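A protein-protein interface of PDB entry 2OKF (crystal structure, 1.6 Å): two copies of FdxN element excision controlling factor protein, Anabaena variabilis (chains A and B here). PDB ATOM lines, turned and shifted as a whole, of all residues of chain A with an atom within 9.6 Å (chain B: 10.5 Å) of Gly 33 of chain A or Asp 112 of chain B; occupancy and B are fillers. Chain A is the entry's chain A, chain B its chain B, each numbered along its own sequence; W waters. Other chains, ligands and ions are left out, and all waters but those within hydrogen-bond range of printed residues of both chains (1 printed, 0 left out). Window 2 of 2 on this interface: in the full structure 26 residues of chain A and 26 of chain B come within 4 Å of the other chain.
Gly 33 of chain A touches just these residues of chain B: Leu 111 (3.8 Å), Asp 112 (3.2 Å) and Phe 113 (2.9 Å).
Asp 112 of chain B touches just one residue of chain A: Gly 33 (3.2 Å).
Val 32 of chain A touches one residue of chain B.
Gly 34 of chain A touches just one residue of chain B: Leu 111.
Val 35 of chain A touches just these residues of chain B: Ile 70, Leu 111 and Pro 114.
Leu 111 of chain B touches just these residues of chain A: Gly 33 (3.8 Å), Gly 34 (3.8 Å) and Val 35 (3.97 Å).
Printed residues of chain A within 4 Å of Pro 114 of chain B: Val 35 (3.7 Å).
Of the printed residues of chain B, Leu 37 of chain A touches Phe 113 (3.96 Å).
Of the printed residues of chain A, Phe 73 of chain B touches Asn 82.
Of the printed residues of chain B, Ala 86 of chain A touches Phe 113 (3.6 Å).
Ile 118 of chain B touches none of the printed residues of chain A.
The nearest residue of chain A that does not touch Asp 112 of chain B is Gly 34 of chain A (5.1 Å).
O of Gly 33 of chain A sits at hydrogen-bond distance from N of Phe 113 of chain B (2.9 Å).
O of Gly 33 of chain A is in hydrogen-bond range of N of Asp 112 of chain B, at 3.2 Å.
NZ of Lys 89 of chain A is in salt-bridge range of OE2 of Glu 120 of chain B (3.7 Å).
Of the 19 printed residues of chain B, 8 touch a printed residue of chain A.
Of the 13 printed residues of chain A, 9 touch a printed residue of chain B.
Hydrophobic or aromatic side chains of chain A within 4 Å of the printed part of chain B: Val 32, Val 35, Leu 37 and Ala 86.
Among the printed residues, 15 pairs touch across the chains.
No position is printed for both chains.
Of the 15 pairs that touch across the chains among the printed residues, none has its exchanged pair printed and touching as well.
O of Val 32 of chain A touches CB of Phe 113 of chain B, at 3.4 Å.
CB of Leu 111 of chain B touches O of Gly 33 of chain A (3.8 Å).
Gly 34 of chain A touches Leu 111 of chain B.
Val 35 of chain A touches Ile 70 of chain B.
Phe 113 of chain B touches Leu 37 of chain A.
Asn 82 of chain A touches Phe 73 of chain B (ND2 to CE2, 3.4 Å).
Asn 82 of chain A touches Phe 113 of chain B (O to CZ, 3.4 Å).
ND2 of Asn 82 of chain A touches CG2 of Ile 117 of chain B (3.3 Å).
Gly 85 of chain A touches Ile 117 of chain B (CA to CD1, 3.9 Å).
Ala 86 of chain A touches Phe 113 of chain B (CB to CE1, 3.6 Å).
The backbone NH of Leu 37 of chain A sits at hydrogen-bond distance from the backbone carbonyl oxygen of Ile 30 of chain A (2.9 Å).
OE2 of Glu 116 of chain B sits close to OE2 of Glu 120 of chain B (2.5 Å).
Water W1 lies within hydrogen-bond range of O of Gly 85 of chain A (2.8 Å), NZ of Lys 89 of chain A (2.8 Å) and OE2 of Glu 120 of chain B (3.0 Å).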
ATOM      1  N   ILE A  30      19.113  -5.613  12.651  1.00  0.00           N
ATOM      2  CA  ILE A  30      19.077  -5.869  11.218  1.00  0.00           C
ATOM      3  C   ILE A  30      17.671  -6.351  10.831  1.00  0.00           C
ATOM      4  O   ILE A  30      17.179  -7.341  11.376  1.00  0.00           O
ATOM      5  CB  ILE A  30      20.122  -6.949  10.827  1.00  0.00           C
ATOM      6  CG1 ILE A  30      21.496  -6.630  11.433  1.00  0.00           C
ATOM      7  CG2 ILE A  30      20.237  -7.090   9.288  1.00  0.00           C
ATOM      8  CD1 ILE A  30      22.503  -7.749  11.287  1.00  0.00           C
ATOM      9  N   SER A  31      17.031  -5.637   9.917  1.00  0.00           N
ATOM     10  CA  SER A  31      15.731  -6.058   9.399  1.00  0.00           C
ATOM     11  C   SER A  31      15.841  -6.175   7.886  1.00  0.00           C
ATOM     12  O   SER A  31      16.221  -5.231   7.215  1.00  0.00           O
ATOM     13  CB  SER A  31      14.637  -5.065   9.789  1.00  0.00           C
ATOM     14  OG  SER A  31      14.363  -5.155  11.184  1.00  0.00           O
ATOM     15  N   VAL A  32      15.549  -7.343   7.325  1.00  0.00           N
ATOM     16  CA  VAL A  32      15.635  -7.450   5.894  1.00  0.00           C
ATOM     17  C   VAL A  32      14.839  -8.635   5.398  1.00  0.00           C
ATOM     18  O   VAL A  32      14.726  -9.660   6.084  1.00  0.00           O
ATOM     19  CB  VAL A  32      17.109  -7.563   5.387  1.00  0.00           C
ATOM     20  CG1 VAL A  32      17.713  -8.832   5.835  1.00  0.00           C
ATOM     21  CG2 VAL A  32      17.182  -7.445   3.853  1.00  0.00           C
ATOM     22  N   GLY A  33      14.249  -8.460   4.224  1.00  0.00           N
ATOM     23  CA  GLY A  33      13.559  -9.539   3.563  1.00  0.00           C
ATOM     24  C   GLY A  33      12.489 -10.215   4.368  1.00  0.00           C
ATOM     25  O   GLY A  33      12.324 -11.425   4.269  1.00  0.00           O
ATOM     26  N   GLY A  34      11.741  -9.418   5.139  1.00  0.00           N
ATOM     27  CA  GLY A  34      10.616  -9.924   5.921  1.00  0.00           C
ATOM     28  C   GLY A  34      10.969 -10.471   7.287  1.00  0.00           C
ATOM     29  O   GLY A  34      10.102 -10.989   7.999  1.00  0.00           O
ATOM     30  N   VAL A  35      12.234 -10.360   7.674  1.00  0.00           N
ATOM     31  CA  VAL A  35      12.667 -10.876   8.949  1.00  0.00           C
ATOM     32  C   VAL A  35      13.443  -9.838   9.761  1.00  0.00           C
ATOM     33  O   VAL A  35      14.218  -9.059   9.218  1.00  0.00           O
ATOM     34  CB  VAL A  35      13.540 -12.153   8.733  1.00  0.00           C
ATOM     35  CG1 VAL A  35      14.047 -12.688  10.035  1.00  0.00           C
ATOM     36  CG2 VAL A  35      12.727 -13.202   8.004  1.00  0.00           C
ATOM     37  N   ASN A  36      13.186  -9.823  11.063  1.00  0.00           N
ATOM     38  CA  ASN A  36      13.908  -8.962  11.987  1.00  0.00           C
ATOM     39  C   ASN A  36      14.817  -9.883  12.763  1.00  0.00           C
ATOM     40  O   ASN A  36      14.351 -10.717  13.538  1.00  0.00           O
ATOM     41  CB  ASN A  36      12.960  -8.215  12.934  1.00  0.00           C
ATOM     42  CG  ASN A  36      13.700  -7.419  14.017  1.00  0.00           C
ATOM     43  OD1 ASN A  36      13.121  -7.094  15.050  1.00  0.00           O
ATOM     44  ND2 ASN A  36      14.977  -7.123  13.789  1.00  0.00           N
ATOM     45  N   LEU A  37      16.110  -9.741  12.535  1.00  0.00           N
ATOM     46  CA  LEU A  37      17.086 -10.582  13.200  1.00  0.00           C
ATOM     47  C   LEU A  37      17.512  -9.972  14.539  1.00  0.00           C
ATOM     48  O   LEU A  37      16.853  -9.054  15.052  1.00  0.00           O
ATOM     49  CB  LEU A  37      18.294 -10.808  12.289  1.00  0.00           C
ATOM     50  CG  LEU A  37      18.052 -11.633  11.020  1.00  0.00           C
ATOM     51  CD1 LEU A  37      17.441 -10.777   9.915  1.00  0.00           C
ATOM     52  CD2 LEU A  37      19.351 -12.214  10.519  1.00  0.00           C
ATOM     53  N   ASN A  82      23.577 -16.374   8.839  1.00  0.00           N
ATOM     54  CA  ASN A  82      22.415 -15.524   8.636  1.00  0.00           C
ATOM     55  C   ASN A  82      22.748 -14.059   8.752  1.00  0.00           C
ATOM     56  O   ASN A  82      22.352 -13.239   7.907  1.00  0.00           O
ATOM     57  CB  ASN A  82      21.312 -15.910   9.611  1.00  0.00           C
ATOM     58  CG  ASN A  82      20.511 -17.117   9.161  1.00  0.00           C
ATOM     59  OD1 ASN A  82      20.032 -17.911   9.982  1.00  0.00           O
ATOM     60  ND2 ASN A  82      20.331 -17.277   7.923  1.00  0.00           N
ATOM     61  N   GLY A  85      24.834 -12.955   5.755  1.00  0.00           N
ATOM     62  CA  GLY A  85      24.034 -12.878   4.554  1.00  0.00           C
ATOM     63  C   GLY A  85      23.128 -11.650   4.582  1.00  0.00           C
ATOM     64  O   GLY A  85      22.917 -10.983   3.566  1.00  0.00           O
ATOM     65  N   ALA A  86      22.569 -11.345   5.755  1.00  0.00           N
ATOM     66  CA  ALA A  86      21.721 -10.164   5.897  1.00  0.00           C
ATOM     67  C   ALA A  86      22.553  -8.879   5.723  1.00  0.00           C
ATOM     68  O   ALA A  86      22.140  -7.950   5.036  1.00  0.00           O
ATOM     69  CB  ALA A  86      21.032 -10.186   7.250  1.00  0.00           C
ATOM     70  N   LYS A  89      23.275  -7.503   2.253  1.00  0.00           N
ATOM     71  CA  LYS A  89      22.143  -6.860   1.617  1.00  0.00           C
ATOM     72  C   LYS A  89      21.621  -5.614   2.338  1.00  0.00           C
ATOM     73  O   LYS A  89      20.667  -4.967   1.852  1.00  0.00           O
ATOM     74  CB  LYS A  89      21.040  -7.903   1.461  1.00  0.00           C
ATOM     75  CG  LYS A  89      21.486  -9.170   0.693  1.00  0.00           C
ATOM     76  CD  LYS A  89      21.715  -8.929  -0.769  1.00  0.00           C
ATOM     77  CE  LYS A  89      22.041 -10.239  -1.507  1.00  0.00           C
ATOM     78  NZ  LYS A  89      23.464 -10.744  -1.266  1.00  0.00           N
ATOM     79  N   VAL A  90      22.284  -5.214   3.419  1.00  0.00           N
ATOM     80  CA  VAL A  90      21.883  -4.051   4.193  1.00  0.00           C
ATOM     81  C   VAL A  90      23.043  -3.059   4.439  1.00  0.00           C
ATOM     82  O   VAL A  90      22.916  -1.859   4.226  1.00  0.00           O
ATOM     83  CB  VAL A  90      21.260  -4.489   5.531  1.00  0.00           C
ATOM     84  CG1 VAL A  90      20.859  -3.262   6.328  1.00  0.00           C
ATOM     85  CG2 VAL A  90      20.035  -5.322   5.268  1.00  0.00           C
ATOM     86  N   ILE B  70      12.944 -17.487  13.259  1.00  0.00           N
ATOM     87  CA  ILE B  70      14.319 -17.095  12.987  1.00  0.00           C
ATOM     88  C   ILE B  70      15.301 -17.742  13.977  1.00  0.00           C
ATOM     89  O   ILE B  70      16.355 -18.189  13.568  1.00  0.00           O
ATOM     90  CB  ILE B  70      14.515 -15.549  12.837  1.00  0.00           C
ATOM     91  CG1 ILE B  70      15.936 -15.192  12.387  1.00  0.00           C
ATOM     92  CG2 ILE B  70      14.218 -14.829  14.115  1.00  0.00           C
ATOM     93  CD1 ILE B  70      16.342 -15.745  11.011  1.00  0.00           C
ATOM     94  N   PHE B  73      15.609 -21.224  12.994  1.00  0.00           N
ATOM     95  CA  PHE B  73      16.352 -21.279  11.750  1.00  0.00           C
ATOM     96  C   PHE B  73      17.849 -21.152  11.959  1.00  0.00           C
ATOM     97  O   PHE B  73      18.621 -21.864  11.348  1.00  0.00           O
ATOM     98  CB  PHE B  73      15.802 -20.266  10.727  1.00  0.00           C
ATOM     99  CG  PHE B  73      16.471 -20.331   9.367  1.00  0.00           C
ATOM    100  CD1 PHE B  73      16.580 -21.540   8.683  1.00  0.00           C
ATOM    101  CD2 PHE B  73      16.977 -19.181   8.759  1.00  0.00           C
ATOM    102  CE1 PHE B  73      17.216 -21.593   7.428  1.00  0.00           C
ATOM    103  CE2 PHE B  73      17.540 -19.231   7.499  1.00  0.00           C
ATOM    104  CZ  PHE B  73      17.674 -20.420   6.847  1.00  0.00           C
ATOM    105  N   THR B 104       5.393 -24.388   7.331  1.00  0.00           N
ATOM    106  CA  THR B 104       6.591 -23.565   7.506  1.00  0.00           C
ATOM    107  C   THR B 104       7.169 -23.168   6.167  1.00  0.00           C
ATOM    108  O   THR B 104       7.610 -22.014   5.956  1.00  0.00           O
ATOM    109  CB  THR B 104       7.628 -24.360   8.267  1.00  0.00           C
ATOM    110  OG1 THR B 104       7.018 -24.916   9.454  1.00  0.00           O
ATOM    111  CG2 THR B 104       8.834 -23.499   8.624  1.00  0.00           C
ATOM    112  N   TYR B 105       7.225 -24.143   5.267  1.00  0.00           N
ATOM    113  CA  TYR B 105       7.735 -23.922   3.916  1.00  0.00           C
ATOM    114  C   TYR B 105       6.950 -22.809   3.185  1.00  0.00           C
ATOM    115  O   TYR B 105       7.517 -21.988   2.514  1.00  0.00           O
ATOM    116  CB  TYR B 105       7.669 -25.239   3.109  1.00  0.00           C
ATOM    117  CG  TYR B 105       8.176 -25.079   1.691  1.00  0.00           C
ATOM    118  CD1 TYR B 105       9.526 -24.821   1.430  1.00  0.00           C
ATOM    119  CD2 TYR B 105       7.314 -25.175   0.630  1.00  0.00           C
ATOM    120  CE1 TYR B 105       9.979 -24.646   0.137  1.00  0.00           C
ATOM    121  CE2 TYR B 105       7.761 -24.996  -0.680  1.00  0.00           C
ATOM    122  CZ  TYR B 105       9.103 -24.747  -0.912  1.00  0.00           C
ATOM    123  OH  TYR B 105       9.560 -24.574  -2.217  1.00  0.00           O
ATOM    124  N   LYS B 106       5.631 -22.832   3.317  1.00  0.00           N
ATOM    125  CA  LYS B 106       4.743 -21.880   2.645  1.00  0.00           C
ATOM    126  C   LYS B 106       4.717 -20.503   3.280  1.00  0.00           C
ATOM    127  O   LYS B 106       4.219 -19.561   2.662  1.00  0.00           O
ATOM    128  CB  LYS B 106       3.317 -22.440   2.562  1.00  0.00           C
ATOM    129  CG  LYS B 106       3.184 -23.667   1.681  1.00  0.00           C
ATOM    130  CD  LYS B 106       1.768 -24.275   1.692  1.00  0.00           C
ATOM    131  CE  LYS B 106       0.793 -23.486   0.908  1.00  0.00           C
ATOM    132  NZ  LYS B 106      -0.453 -24.288   0.852  1.00  0.00           N
ATOM    133  N   THR B 107       5.215 -20.379   4.506  1.00  0.00           N
ATOM    134  CA  THR B 107       5.192 -19.111   5.222  1.00  0.00           C
ATOM    135  C   THR B 107       6.620 -18.571   5.409  1.00  0.00           C
ATOM    136  O   THR B 107       7.109 -17.783   4.586  1.00  0.00           O
ATOM    137  CB  THR B 107       4.429 -19.259   6.533  1.00  0.00           C
ATOM    138  OG1 THR B 107       4.976 -20.296   7.356  1.00  0.00           O
ATOM    139  CG2 THR B 107       3.008 -19.601   6.235  1.00  0.00           C
ATOM    140  N   PHE B 108       7.303 -19.038   6.447  1.00  0.00           N
ATOM    141  CA  PHE B 108       8.624 -18.567   6.751  1.00  0.00           C
ATOM    142  C   PHE B 108       9.556 -18.700   5.556  1.00  0.00           C
ATOM    143  O   PHE B 108      10.290 -17.786   5.226  1.00  0.00           O
ATOM    144  CB  PHE B 108       9.192 -19.337   7.940  1.00  0.00           C
ATOM    145  CG  PHE B 108      10.575 -18.892   8.353  1.00  0.00           C
ATOM    146  CD1 PHE B 108      10.735 -17.699   9.000  1.00  0.00           C
ATOM    147  CD2 PHE B 108      11.696 -19.664   8.115  1.00  0.00           C
ATOM    148  CE1 PHE B 108      12.010 -17.281   9.379  1.00  0.00           C
ATOM    149  CE2 PHE B 108      12.948 -19.229   8.491  1.00  0.00           C
ATOM    150  CZ  PHE B 108      13.080 -18.049   9.140  1.00  0.00           C
ATOM    151  N   PHE B 109       9.577 -19.861   4.916  1.00  0.00           N
ATOM    152  CA  PHE B 109      10.506 -20.036   3.814  1.00  0.00           C
ATOM    153  C   PHE B 109      10.122 -19.345   2.493  1.00  0.00           C
ATOM    154  O   PHE B 109      10.917 -19.399   1.554  1.00  0.00           O
ATOM    155  CB  PHE B 109      10.888 -21.485   3.624  1.00  0.00           C
ATOM    156  CG  PHE B 109      11.770 -22.002   4.718  1.00  0.00           C
ATOM    157  CD1 PHE B 109      13.087 -21.576   4.807  1.00  0.00           C
ATOM    158  CD2 PHE B 109      11.277 -22.826   5.714  1.00  0.00           C
ATOM    159  CE1 PHE B 109      13.886 -22.002   5.855  1.00  0.00           C
ATOM    160  CE2 PHE B 109      12.072 -23.260   6.745  1.00  0.00           C
ATOM    161  CZ  PHE B 109      13.395 -22.887   6.796  1.00  0.00           C
ATOM    162  N   GLN B 110       8.972 -18.681   2.451  1.00  0.00           N
ATOM    163  CA  GLN B 110       8.609 -17.822   1.321  1.00  0.00           C
ATOM    164  C   GLN B 110       8.948 -16.371   1.586  1.00  0.00           C
ATOM    165  O   GLN B 110       8.828 -15.533   0.693  1.00  0.00           O
ATOM    166  CB  GLN B 110       7.144 -17.989   0.911  1.00  0.00           C
ATOM    167  CG  GLN B 110       6.842 -19.447   0.523  1.00  0.00           C
ATOM    168  CD  GLN B 110       7.842 -20.002  -0.469  1.00  0.00           C
ATOM    169  OE1 GLN B 110       8.102 -19.371  -1.494  1.00  0.00           O
ATOM    170  NE2 GLN B 110       8.446 -21.146  -0.158  1.00  0.00           N
ATOM    171  N   LEU B 111       9.365 -16.041   2.805  1.00  0.00           N
ATOM    172  CA  LEU B 111       9.847 -14.715   3.076  1.00  0.00           C
ATOM    173  C   LEU B 111      11.175 -14.568   2.307  1.00  0.00           C
ATOM    174  O   LEU B 111      11.928 -15.532   2.147  1.00  0.00           O
ATOM    175  CB  LEU B 111      10.046 -14.476   4.571  1.00  0.00           C
ATOM    176  CG  LEU B 111       8.778 -14.521   5.410  1.00  0.00           C
ATOM    177  CD1 LEU B 111       9.154 -14.521   6.879  1.00  0.00           C
ATOM    178  CD2 LEU B 111       7.864 -13.364   5.060  1.00  0.00           C
ATOM    179  N   ASP B 112      11.454 -13.355   1.842  1.00  0.00           N
ATOM    180  CA  ASP B 112      12.607 -13.107   1.002  1.00  0.00           C
ATOM    181  C   ASP B 112      13.940 -13.518   1.641  1.00  0.00           C
ATOM    182  O   ASP B 112      14.741 -14.177   1.003  1.00  0.00           O
ATOM    183  CB  ASP B 112      12.670 -11.642   0.593  1.00  0.00           C
ATOM    184  CG  ASP B 112      11.593 -11.229  -0.419  1.00  0.00           C
ATOM    185  OD1 ASP B 112      10.933 -12.090  -1.007  1.00  0.00           O
ATOM    186  OD2 ASP B 112      11.473 -10.010  -0.623  1.00  0.00           O
ATOM    187  N   PHE B 113      14.143 -13.184   2.903  1.00  0.00           N
ATOM    188  CA  PHE B 113      15.439 -13.473   3.519  1.00  0.00           C
ATOM    189  C   PHE B 113      15.698 -14.966   3.677  1.00  0.00           C
ATOM    190  O   PHE B 113      16.716 -15.452   3.208  1.00  0.00           O
ATOM    191  CB  PHE B 113      15.596 -12.703   4.827  1.00  0.00           C
ATOM    192  CG  PHE B 113      16.815 -13.069   5.572  1.00  0.00           C
ATOM    193  CD1 PHE B 113      18.021 -12.578   5.183  1.00  0.00           C
ATOM    194  CD2 PHE B 113      16.768 -14.000   6.587  1.00  0.00           C
ATOM    195  CE1 PHE B 113      19.173 -12.924   5.869  1.00  0.00           C
ATOM    196  CE2 PHE B 113      17.931 -14.374   7.269  1.00  0.00           C
ATOM    197  CZ  PHE B 113      19.106 -13.833   6.908  1.00  0.00           C
ATOM    198  N   PRO B 114      14.799 -15.718   4.352  1.00  0.00           N
ATOM    199  CA  PRO B 114      15.096 -17.153   4.496  1.00  0.00           C
ATOM    200  C   PRO B 114      15.200 -17.857   3.165  1.00  0.00           C
ATOM    201  O   PRO B 114      16.051 -18.741   3.008  1.00  0.00           O
ATOM    202  CB  PRO B 114      13.878 -17.685   5.273  1.00  0.00           C
ATOM    203  CG  PRO B 114      13.280 -16.549   5.897  1.00  0.00           C
ATOM    204  CD  PRO B 114      13.591 -15.325   5.091  1.00  0.00           C
ATOM    205  N   LYS B 115      14.328 -17.475   2.233  1.00  0.00           N
ATOM    206  CA  LYS B 115      14.389 -18.080   0.923  1.00  0.00           C
ATOM    207  C   LYS B 115      15.799 -17.894   0.335  1.00  0.00           C
ATOM    208  O   LYS B 115      16.417 -18.817  -0.172  1.00  0.00           O
ATOM    209  CB  LYS B 115      13.321 -17.480  -0.007  1.00  0.00           C
ATOM    210  CG  LYS B 115      13.384 -18.013  -1.431  1.00  0.00           C
ATOM    211  CD  LYS B 115      12.305 -17.379  -2.331  1.00  0.00           C
ATOM    212  CE  LYS B 115      10.920 -17.887  -2.007  1.00  0.00           C
ATOM    213  N   GLU B 116      16.303 -16.677   0.404  1.00  0.00           N
ATOM    214  CA  GLU B 116      17.632 -16.364  -0.154  1.00  0.00           C
ATOM    215  C   GLU B 116      18.762 -17.105   0.568  1.00  0.00           C
ATOM    216  O   GLU B 116      19.676 -17.608  -0.058  1.00  0.00           O
ATOM    217  CB  GLU B 116      17.846 -14.854  -0.196  1.00  0.00           C
ATOM    218  CG  GLU B 116      19.213 -14.380  -0.650  1.00  0.00           C
ATOM    219  CD  GLU B 116      19.489 -14.639  -2.127  1.00  0.00           C
ATOM    220  OE1 GLU B 116      18.545 -14.875  -2.889  1.00  0.00           O
ATOM    221  OE2 GLU B 116      20.687 -14.520  -2.510  1.00  0.00           O
ATOM    222  N   ILE B 117      18.730 -17.129   1.897  1.00  0.00           N
ATOM    223  CA  ILE B 117      19.783 -17.820   2.628  1.00  0.00           C
ATOM    224  C   ILE B 117      19.828 -19.300   2.289  1.00  0.00           C
ATOM    225  O   ILE B 117      20.902 -19.889   2.104  1.00  0.00           O
ATOM    226  CB  ILE B 117      19.607 -17.634   4.139  1.00  0.00           C
ATOM    227  CG1 ILE B 117      19.852 -16.201   4.523  1.00  0.00           C
ATOM    228  CG2 ILE B 117      20.523 -18.628   4.921  1.00  0.00           C
ATOM    229  CD1 ILE B 117      21.326 -15.692   4.298  1.00  0.00           C
ATOM    230  N   ILE B 118      18.661 -19.929   2.189  1.00  0.00           N
ATOM    231  CA  ILE B 118      18.583 -21.352   1.829  1.00  0.00           C
ATOM    232  C   ILE B 118      19.263 -21.590   0.491  1.00  0.00           C
ATOM    233  O   ILE B 118      20.067 -22.520   0.345  1.00  0.00           O
ATOM    234  CB  ILE B 118      17.128 -21.789   1.734  1.00  0.00           C
ATOM    235  CG1 ILE B 118      16.522 -21.934   3.133  1.00  0.00           C
ATOM    236  CG2 ILE B 118      16.969 -23.073   0.942  1.00  0.00           C
ATOM    237  CD1 ILE B 118      17.023 -23.069   3.947  1.00  0.00           C
ATOM    238  N   ILE B 119      18.958 -20.744  -0.489  1.00  0.00           N
ATOM    239  CA  ILE B 119      19.537 -20.895  -1.813  1.00  0.00           C
ATOM    240  C   ILE B 119      21.016 -20.570  -1.807  1.00  0.00           C
ATOM    241  O   ILE B 119      21.828 -21.270  -2.436  1.00  0.00           O
ATOM    242  CB  ILE B 119      18.764 -20.060  -2.865  1.00  0.00           C
ATOM    243  CG1 ILE B 119      17.321 -20.522  -2.918  1.00  0.00           C
ATOM    244  CG2 ILE B 119      19.424 -20.190  -4.216  1.00  0.00           C
ATOM    245  CD1 ILE B 119      16.400 -19.468  -3.543  1.00  0.00           C
ATOM    246  N   GLU B 120      21.417 -19.525  -1.076  1.00  0.00           N
ATOM    247  CA  GLU B 120      22.822 -19.178  -1.072  1.00  0.00           C
ATOM    248  C   GLU B 120      23.698 -20.267  -0.511  1.00  0.00           C
ATOM    249  O   GLU B 120      24.897 -20.325  -0.783  1.00  0.00           O
ATOM    250  CB  GLU B 120      23.070 -17.874  -0.303  1.00  0.00           C
ATOM    251  CG  GLU B 120      22.541 -16.600  -0.923  1.00  0.00           C
ATOM    252  CD  GLU B 120      22.829 -15.296  -0.172  1.00  0.00           C
ATOM    253  OE1 GLU B 120      23.529 -15.322   0.843  1.00  0.00           O
ATOM    254  OE2 GLU B 120      22.340 -14.226  -0.654  1.00  0.00           O
HETATM  255  O   HOH W   1      23.568 -12.192   1.175  1.00  0.00           O
